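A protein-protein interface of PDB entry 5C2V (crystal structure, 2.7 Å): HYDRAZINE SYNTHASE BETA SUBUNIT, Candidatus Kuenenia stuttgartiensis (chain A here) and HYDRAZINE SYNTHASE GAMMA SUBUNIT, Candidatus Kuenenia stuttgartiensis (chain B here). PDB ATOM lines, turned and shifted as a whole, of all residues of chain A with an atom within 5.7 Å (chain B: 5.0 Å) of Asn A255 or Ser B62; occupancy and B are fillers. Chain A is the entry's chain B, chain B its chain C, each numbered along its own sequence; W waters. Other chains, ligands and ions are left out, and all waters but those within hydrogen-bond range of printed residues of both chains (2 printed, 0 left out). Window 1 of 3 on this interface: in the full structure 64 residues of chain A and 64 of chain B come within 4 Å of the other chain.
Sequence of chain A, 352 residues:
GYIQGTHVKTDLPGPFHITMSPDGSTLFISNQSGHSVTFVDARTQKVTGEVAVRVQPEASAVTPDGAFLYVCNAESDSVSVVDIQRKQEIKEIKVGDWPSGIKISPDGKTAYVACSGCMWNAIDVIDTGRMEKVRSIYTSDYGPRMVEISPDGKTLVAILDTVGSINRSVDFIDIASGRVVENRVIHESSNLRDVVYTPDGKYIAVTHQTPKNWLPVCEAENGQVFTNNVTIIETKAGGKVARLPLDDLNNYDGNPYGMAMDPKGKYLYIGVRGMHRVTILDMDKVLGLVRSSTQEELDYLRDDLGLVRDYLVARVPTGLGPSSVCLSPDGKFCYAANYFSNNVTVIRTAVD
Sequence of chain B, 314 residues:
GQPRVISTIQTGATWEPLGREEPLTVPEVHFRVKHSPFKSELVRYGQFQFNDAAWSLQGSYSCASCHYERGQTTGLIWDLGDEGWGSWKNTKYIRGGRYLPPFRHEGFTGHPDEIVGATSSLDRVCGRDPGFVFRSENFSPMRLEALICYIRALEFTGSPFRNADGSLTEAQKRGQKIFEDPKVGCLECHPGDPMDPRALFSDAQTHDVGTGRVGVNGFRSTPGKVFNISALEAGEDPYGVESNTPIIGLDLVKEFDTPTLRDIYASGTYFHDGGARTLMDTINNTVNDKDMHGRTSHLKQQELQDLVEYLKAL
The side-chain amide nitrogen (ND2) of Asn A191 sits at hydrogen-bond distance from the backbone carbonyl oxygen (O) of Ser B65.
OE1 of Gln A209 is in hydrogen-bond range of OG of Ser B65.
The backbone carbonyl oxygen (O) of Ser B60 sits at hydrogen-bond distance from the side-chain amide nitrogen (ND2) of Asn A228, 3.0 Å away.
OG of Ser B62 is in hydrogen-bond range of OD1 of Asn A255 (3.1 Å).
The side-chain amide nitrogen of Asn A255 lies within hydrogen-bond range of the side-chain hydroxyl of Ser B65 (2.7 Å).
The guanidinium group (NH1) of Arg A273 sits at hydrogen-bond distance from the side-chain amide oxygen (OD1) of Asn B51, 3.1 Å away.
The backbone carbonyl oxygen (O) of Gly A274 sits at hydrogen-bond distance from the backbone NH (N) of Ala B53, at 3.2 Å.
The backbone carbonyl oxygen of Gly A274 sits close to the side-chain carboxylate of Asp B52, 3.3 Å away.
Of the printed residues of chain B, Asn A255 touches Ser B62 and Ser B65.
Printed residues of chain B within 4 Å of Arg A273: Asn B51 (3.1 Å).
Printed residues of chain B within 4 Å of Gly A274: Asp B52 and Ala B53.
Ser B62 touches just one residue of chain A: Asn A255.
The nearest printed residue of chain B that does not touch Asn A191 is Ala B64 (4.7 Å).
Among the printed residues, pairs that only touch across the chains: Gln A209 with Ser B60.
Of the 12 printed residues of chain A, 6 touch a printed residue of chain B.
Printed residues of chain A that touch a printed residue of chain B: Asn A191, Gln A209, Asn A228, Asn A255, Arg A273 and Gly A274.
Of the 12 printed residues of chain B, 6 touch a printed residue of chain A.
Hydrophobic or aromatic side chains of chain B that line the printed part of chain A: Ala B53.
Among the printed residues, 9 pairs touch across the chains.
Water W2 bridges the backbone carbonyl oxygen of Ala B64 (2.6 Å) and the side-chain amide oxygen of Asn A191 (3.2 Å).
Water W1 lies within hydrogen-bond range of the side-chain hydroxyl of Tyr A257 (2.8 Å), the guanidinium group of Arg A273 (3.0 Å) and the side-chain amide oxygen of Asn B51 (3.2 Å).
OD1 of Asn A228 sits at hydrogen-bond distance from NE2 of Gln A209 (2.7 Å).
The side-chain amide nitrogen of Gln A209 sits close to the side-chain amide nitrogen of Asn A255 (3.2 Å).
The backbone NH (N) of Gly A274 sits at hydrogen-bond distance from the backbone carbonyl oxygen (O) of Gly A254.
N of Arg A273 is in hydrogen-bond range of O of Asn A255, 3.3 Å away.
The side-chain hydroxyl (OG) of Ser B62 lies close to the backbone NH (N) of Ala B64 (3.3 Å).
N of Ser B62 lies within hydrogen-bond range of OG of Ser B65 (3.1 Å).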
ATOM      1  N   ASN A 191     -32.238  32.941 -10.501  1.00  0.00           N
ATOM      2  CA  ASN A 191     -30.848  32.624 -10.180  1.00  0.00           C
ATOM      3  C   ASN A 191     -30.082  31.906 -11.290  1.00  0.00           C
ATOM      4  O   ASN A 191     -29.560  30.814 -11.062  1.00  0.00           O
ATOM      5  CB  ASN A 191     -30.775  31.777  -8.905  1.00  0.00           C
ATOM      6  CG  ASN A 191     -31.466  32.430  -7.728  1.00  0.00           C
ATOM      7  OD1 ASN A 191     -31.457  33.652  -7.587  1.00  0.00           O
ATOM      8  ND2 ASN A 191     -32.068  31.614  -6.868  1.00  0.00           N
ATOM      9  N   GLN A 209     -32.921  27.873 -11.000  1.00  0.00           N
ATOM     10  CA  GLN A 209     -33.933  27.358 -10.089  1.00  0.00           C
ATOM     11  C   GLN A 209     -35.335  27.712 -10.565  1.00  0.00           C
ATOM     12  O   GLN A 209     -35.538  28.719 -11.242  1.00  0.00           O
ATOM     13  CB  GLN A 209     -33.718  27.902  -8.674  1.00  0.00           C
ATOM     14  CG  GLN A 209     -32.600  27.228  -7.903  1.00  0.00           C
ATOM     15  CD  GLN A 209     -32.544  27.677  -6.456  1.00  0.00           C
ATOM     16  OE1 GLN A 209     -32.621  28.869  -6.161  1.00  0.00           O
ATOM     17  NE2 GLN A 209     -32.416  26.720  -5.544  1.00  0.00           N
ATOM     18  N   ASN A 228     -34.756  22.582  -8.478  1.00  0.00           N
ATOM     19  CA  ASN A 228     -33.509  22.967  -9.123  1.00  0.00           C
ATOM     20  C   ASN A 228     -33.377  22.336 -10.498  1.00  0.00           C
ATOM     21  O   ASN A 228     -33.538  21.125 -10.653  1.00  0.00           O
ATOM     22  CB  ASN A 228     -32.331  22.591  -8.240  1.00  0.00           C
ATOM     23  CG  ASN A 228     -32.394  23.263  -6.884  1.00  0.00           C
ATOM     24  OD1 ASN A 228     -31.869  24.360  -6.698  1.00  0.00           O
ATOM     25  ND2 ASN A 228     -33.026  22.599  -5.923  1.00  0.00           N
ATOM     26  N   ASP A 253     -30.680  19.156  -5.568  1.00  0.00           N
ATOM     27  CA  ASP A 253     -29.381  19.799  -5.702  1.00  0.00           C
ATOM     28  C   ASP A 253     -29.553  21.286  -5.451  1.00  0.00           C
ATOM     29  O   ASP A 253     -30.001  22.009  -6.327  1.00  0.00           O
ATOM     30  CB  ASP A 253     -28.802  19.578  -7.105  1.00  0.00           C
ATOM     31  CG  ASP A 253     -28.315  18.163  -7.327  1.00  0.00           C
ATOM     32  OD1 ASP A 253     -27.806  17.549  -6.371  1.00  0.00           O
ATOM     33  OD2 ASP A 253     -28.436  17.664  -8.467  1.00  0.00           O
ATOM     34  N   GLY A 254     -29.118  21.755  -4.288  1.00  0.00           N
ATOM     35  CA  GLY A 254     -29.332  23.141  -3.916  1.00  0.00           C
ATOM     36  C   GLY A 254     -28.485  24.111  -4.711  1.00  0.00           C
ATOM     37  O   GLY A 254     -27.262  23.986  -4.726  1.00  0.00           O
ATOM     38  N   ASN A 255     -29.130  25.090  -5.340  1.00  0.00           N
ATOM     39  CA  ASN A 255     -28.422  26.179  -6.009  1.00  0.00           C
ATOM     40  C   ASN A 255     -27.319  25.713  -6.962  1.00  0.00           C
ATOM     41  O   ASN A 255     -26.139  25.822  -6.636  1.00  0.00           O
ATOM     42  CB  ASN A 255     -27.824  27.126  -4.965  1.00  0.00           C
ATOM     43  CG  ASN A 255     -28.854  27.624  -3.971  1.00  0.00           C
ATOM     44  OD1 ASN A 255     -28.742  27.380  -2.769  1.00  0.00           O
ATOM     45  ND2 ASN A 255     -29.861  28.335  -4.466  1.00  0.00           N
ATOM     46  N   PRO A 256     -27.695  25.154  -8.122  1.00  0.00           N
ATOM     47  CA  PRO A 256     -26.671  24.776  -9.103  1.00  0.00           C
ATOM     48  C   PRO A 256     -25.977  26.015  -9.667  1.00  0.00           C
ATOM     49  O   PRO A 256     -26.663  26.979 -10.001  1.00  0.00           O
ATOM     50  CB  PRO A 256     -27.475  24.046 -10.182  1.00  0.00           C
ATOM     51  CG  PRO A 256     -28.839  24.652 -10.095  1.00  0.00           C
ATOM     52  CD  PRO A 256     -29.061  24.938  -8.632  1.00  0.00           C
ATOM     53  N   TYR A 257     -24.649  26.001  -9.769  1.00  0.00           N
ATOM     54  CA  TYR A 257     -23.932  27.207 -10.187  1.00  0.00           C
ATOM     55  C   TYR A 257     -23.083  27.058 -11.440  1.00  0.00           C
ATOM     56  O   TYR A 257     -23.465  27.508 -12.519  1.00  0.00           O
ATOM     57  CB  TYR A 257     -23.018  27.684  -9.057  1.00  0.00           C
ATOM     58  CG  TYR A 257     -23.638  28.687  -8.118  1.00  0.00           C
ATOM     59  CD1 TYR A 257     -24.796  28.384  -7.420  1.00  0.00           C
ATOM     60  CD2 TYR A 257     -23.049  29.926  -7.907  1.00  0.00           C
ATOM     61  CE1 TYR A 257     -25.362  29.291  -6.551  1.00  0.00           C
ATOM     62  CE2 TYR A 257     -23.606  30.842  -7.036  1.00  0.00           C
ATOM     63  CZ  TYR A 257     -24.766  30.518  -6.362  1.00  0.00           C
ATOM     64  OH  TYR A 257     -25.334  31.420  -5.493  1.00  0.00           O
ATOM     65  N   GLY A 271     -21.512  22.250 -10.789  1.00  0.00           N
ATOM     66  CA  GLY A 271     -21.233  22.557  -9.402  1.00  0.00           C
ATOM     67  C   GLY A 271     -22.526  22.824  -8.656  1.00  0.00           C
ATOM     68  O   GLY A 271     -23.302  23.704  -9.034  1.00  0.00           O
ATOM     69  N   VAL A 272     -22.756  22.068  -7.591  1.00  0.00           N
ATOM     70  CA  VAL A 272     -23.911  22.281  -6.733  1.00  0.00           C
ATOM     71  C   VAL A 272     -23.417  22.846  -5.414  1.00  0.00           C
ATOM     72  O   VAL A 272     -22.818  22.134  -4.594  1.00  0.00           O
ATOM     73  CB  VAL A 272     -24.704  20.984  -6.490  1.00  0.00           C
ATOM     74  CG1 VAL A 272     -25.989  21.285  -5.747  1.00  0.00           C
ATOM     75  CG2 VAL A 272     -25.002  20.289  -7.811  1.00  0.00           C
ATOM     76  N   ARG A 273     -23.709  24.128  -5.224  1.00  0.00           N
ATOM     77  CA  ARG A 273     -23.112  24.947  -4.178  1.00  0.00           C
ATOM     78  C   ARG A 273     -23.763  24.714  -2.822  1.00  0.00           C
ATOM     79  O   ARG A 273     -23.081  24.628  -1.801  1.00  0.00           O
ATOM     80  CB  ARG A 273     -23.215  26.422  -4.572  1.00  0.00           C
ATOM     81  CG  ARG A 273     -22.262  27.356  -3.853  1.00  0.00           C
ATOM     82  CD  ARG A 273     -22.504  28.790  -4.300  1.00  0.00           C
ATOM     83  NE  ARG A 273     -21.411  29.682  -3.928  1.00  0.00           N
ATOM     84  CZ  ARG A 273     -21.365  30.374  -2.795  1.00  0.00           C
ATOM     85  NH1 ARG A 273     -22.354  30.278  -1.918  1.00  0.00           N
ATOM     86  NH2 ARG A 273     -20.330  31.163  -2.539  1.00  0.00           N
ATOM     87  N   GLY A 274     -25.087  24.617  -2.820  1.00  0.00           N
ATOM     88  CA  GLY A 274     -25.830  24.396  -1.595  1.00  0.00           C
ATOM     89  C   GLY A 274     -25.612  23.003  -1.041  1.00  0.00           C
ATOM     90  O   GLY A 274     -25.484  22.818   0.170  1.00  0.00           O
ATOM     91  N   PHE B  50     -25.877  30.910   5.853  1.00  0.00           N
ATOM     92  CA  PHE B  50     -26.688  31.679   4.920  1.00  0.00           C
ATOM     93  C   PHE B  50     -26.745  31.005   3.548  1.00  0.00           C
ATOM     94  O   PHE B  50     -27.803  30.952   2.919  1.00  0.00           O
ATOM     95  CB  PHE B  50     -26.133  33.102   4.796  1.00  0.00           C
ATOM     96  CG  PHE B  50     -26.904  33.984   3.854  1.00  0.00           C
ATOM     97  CD1 PHE B  50     -28.051  34.637   4.275  1.00  0.00           C
ATOM     98  CD2 PHE B  50     -26.470  34.177   2.552  1.00  0.00           C
ATOM     99  CE1 PHE B  50     -28.760  35.453   3.412  1.00  0.00           C
ATOM    100  CE2 PHE B  50     -27.174  34.992   1.685  1.00  0.00           C
ATOM    101  CZ  PHE B  50     -28.320  35.631   2.115  1.00  0.00           C
ATOM    102  N   ASN B  51     -25.607  30.496   3.084  1.00  0.00           N
ATOM    103  CA  ASN B  51     -25.536  29.895   1.752  1.00  0.00           C
ATOM    104  C   ASN B  51     -25.749  28.379   1.697  1.00  0.00           C
ATOM    105  O   ASN B  51     -25.869  27.811   0.610  1.00  0.00           O
ATOM    106  CB  ASN B  51     -24.189  30.234   1.109  1.00  0.00           C
ATOM    107  CG  ASN B  51     -24.063  31.703   0.761  1.00  0.00           C
ATOM    108  OD1 ASN B  51     -24.322  32.110  -0.373  1.00  0.00           O
ATOM    109  ND2 ASN B  51     -23.668  32.512   1.739  1.00  0.00           N
ATOM    110  N   ASP B  52     -25.806  27.726   2.854  1.00  0.00           N
ATOM    111  CA  ASP B  52     -25.900  26.265   2.899  1.00  0.00           C
ATOM    112  C   ASP B  52     -27.319  25.753   2.665  1.00  0.00           C
ATOM    113  O   ASP B  52     -28.264  26.221   3.295  1.00  0.00           O
ATOM    114  CB  ASP B  52     -25.389  25.741   4.244  1.00  0.00           C
ATOM    115  CG  ASP B  52     -25.522  24.237   4.369  1.00  0.00           C
ATOM    116  OD1 ASP B  52     -25.273  23.536   3.367  1.00  0.00           O
ATOM    117  OD2 ASP B  52     -25.880  23.756   5.466  1.00  0.00           O
ATOM    118  N   ALA B  53     -27.470  24.814   1.734  1.00  0.00           N
ATOM    119  CA  ALA B  53     -28.752  24.143   1.533  1.00  0.00           C
ATOM    120  C   ALA B  53     -28.822  22.767   2.202  1.00  0.00           C
ATOM    121  O   ALA B  53     -29.875  22.133   2.209  1.00  0.00           O
ATOM    122  CB  ALA B  53     -29.047  24.010   0.047  1.00  0.00           C
ATOM    123  N   SER B  60     -33.540  21.539  -0.745  1.00  0.00           N
ATOM    124  CA  SER B  60     -34.214  22.248  -1.830  1.00  0.00           C
ATOM    125  C   SER B  60     -33.615  23.627  -2.113  1.00  0.00           C
ATOM    126  O   SER B  60     -33.341  23.962  -3.266  1.00  0.00           O
ATOM    127  CB  SER B  60     -35.706  22.388  -1.515  1.00  0.00           C
ATOM    128  OG  SER B  60     -36.391  23.055  -2.559  1.00  0.00           O
ATOM    129  N   TYR B  61     -33.419  24.426  -1.068  1.00  0.00           N
ATOM    130  CA  TYR B  61     -32.898  25.781  -1.240  1.00  0.00           C
ATOM    131  C   TYR B  61     -32.240  26.321   0.027  1.00  0.00           C
ATOM    132  O   TYR B  61     -32.207  25.650   1.059  1.00  0.00           O
ATOM    133  CB  TYR B  61     -34.018  26.727  -1.684  1.00  0.00           C
ATOM    134  CG  TYR B  61     -35.203  26.762  -0.745  1.00  0.00           C
ATOM    135  CD1 TYR B  61     -36.246  25.854  -0.877  1.00  0.00           C
ATOM    136  CD2 TYR B  61     -35.283  27.706   0.270  1.00  0.00           C
ATOM    137  CE1 TYR B  61     -37.329  25.880  -0.021  1.00  0.00           C
ATOM    138  CE2 TYR B  61     -36.364  27.741   1.131  1.00  0.00           C
ATOM    139  CZ  TYR B  61     -37.383  26.827   0.979  1.00  0.00           C
ATOM    140  OH  TYR B  61     -38.463  26.857   1.832  1.00  0.00           O
ATOM    141  N   SER B  62     -31.722  27.541  -0.063  1.00  0.00           N
ATOM    142  CA  SER B  62     -31.079  28.194   1.071  1.00  0.00           C
ATOM    143  C   SER B  62     -31.595  29.620   1.217  1.00  0.00           C
ATOM    144  O   SER B  62     -32.497  30.034   0.488  1.00  0.00           O
ATOM    145  CB  SER B  62     -29.557  28.196   0.903  1.00  0.00           C
ATOM    146  OG  SER B  62     -29.168  28.986  -0.207  1.00  0.00           O
ATOM    147  N   CYS B  63     -31.032  30.362   2.165  1.00  0.00           N
ATOM    148  CA  CYS B  63     -31.366  31.773   2.319  1.00  0.00           C
ATOM    149  C   CYS B  63     -31.016  32.515   1.036  1.00  0.00           C
ATOM    150  O   CYS B  63     -31.785  33.343   0.544  1.00  0.00           O
ATOM    151  CB  CYS B  63     -30.621  32.387   3.505  1.00  0.00           C
ATOM    152  SG  CYS B  63     -30.875  31.553   5.086  1.00  0.00           S
ATOM    153  N   ALA B  64     -29.852  32.179   0.488  1.00  0.00           N
ATOM    154  CA  ALA B  64     -29.326  32.831  -0.703  1.00  0.00           C
ATOM    155  C   ALA B  64     -30.182  32.591  -1.943  1.00  0.00           C
ATOM    156  O   ALA B  64     -29.983  33.226  -2.969  1.00  0.00           O
ATOM    157  CB  ALA B  64     -27.898  32.376  -0.957  1.00  0.00           C
ATOM    158  N   SER B  65     -31.124  31.663  -1.866  1.00  0.00           N
ATOM    159  CA  SER B  65     -32.020  31.441  -2.992  1.00  0.00           C
ATOM    160  C   SER B  65     -33.006  32.605  -3.112  1.00  0.00           C
ATOM    161  O   SER B  65     -33.544  32.871  -4.187  1.00  0.00           O
ATOM    162  CB  SER B  65     -32.761  30.114  -2.836  1.00  0.00           C
ATOM    163  OG  SER B  65     -31.849  29.030  -2.822  1.00  0.00           O
ATOM    164  N   CYS B  66     -33.211  33.305  -1.999  1.00  0.00           N
ATOM    165  CA  CYS B  66     -34.133  34.440  -1.927  1.00  0.00           C
ATOM    166  C   CYS B  66     -33.398  35.786  -1.877  1.00  0.00           C
ATOM    167  O   CYS B  66     -33.603  36.649  -2.731  1.00  0.00           O
ATOM    168  CB  CYS B  66     -35.055  34.302  -0.713  1.00  0.00           C
ATOM    169  SG  CYS B  66     -36.477  33.207  -0.980  1.00  0.00           S
ATOM    170  N   PHE B 134     -38.453  27.117   5.788  1.00  0.00           N
ATOM    171  CA  PHE B 134     -37.679  25.971   5.323  1.00  0.00           C
ATOM    172  C   PHE B 134     -38.305  24.644   5.739  1.00  0.00           C
ATOM    173  O   PHE B 134     -38.110  23.626   5.073  1.00  0.00           O
ATOM    174  CB  PHE B 134     -36.244  26.047   5.853  1.00  0.00           C
ATOM    175  CG  PHE B 134     -35.396  27.087   5.178  1.00  0.00           C
ATOM    176  CD1 PHE B 134     -35.378  28.395   5.636  1.00  0.00           C
ATOM    177  CD2 PHE B 134     -34.603  26.753   4.092  1.00  0.00           C
ATOM    178  CE1 PHE B 134     -34.592  29.351   5.017  1.00  0.00           C
ATOM    179  CE2 PHE B 134     -33.814  27.703   3.471  1.00  0.00           C
ATOM    180  CZ  PHE B 134     -33.809  29.004   3.934  1.00  0.00           C
HETATM  181  O   HOH W   1     -25.237  30.394  -2.877  1.00  0.00           O
HETATM  182  O   HOH W   2     -29.154  33.495  -5.429  1.00  0.00           O
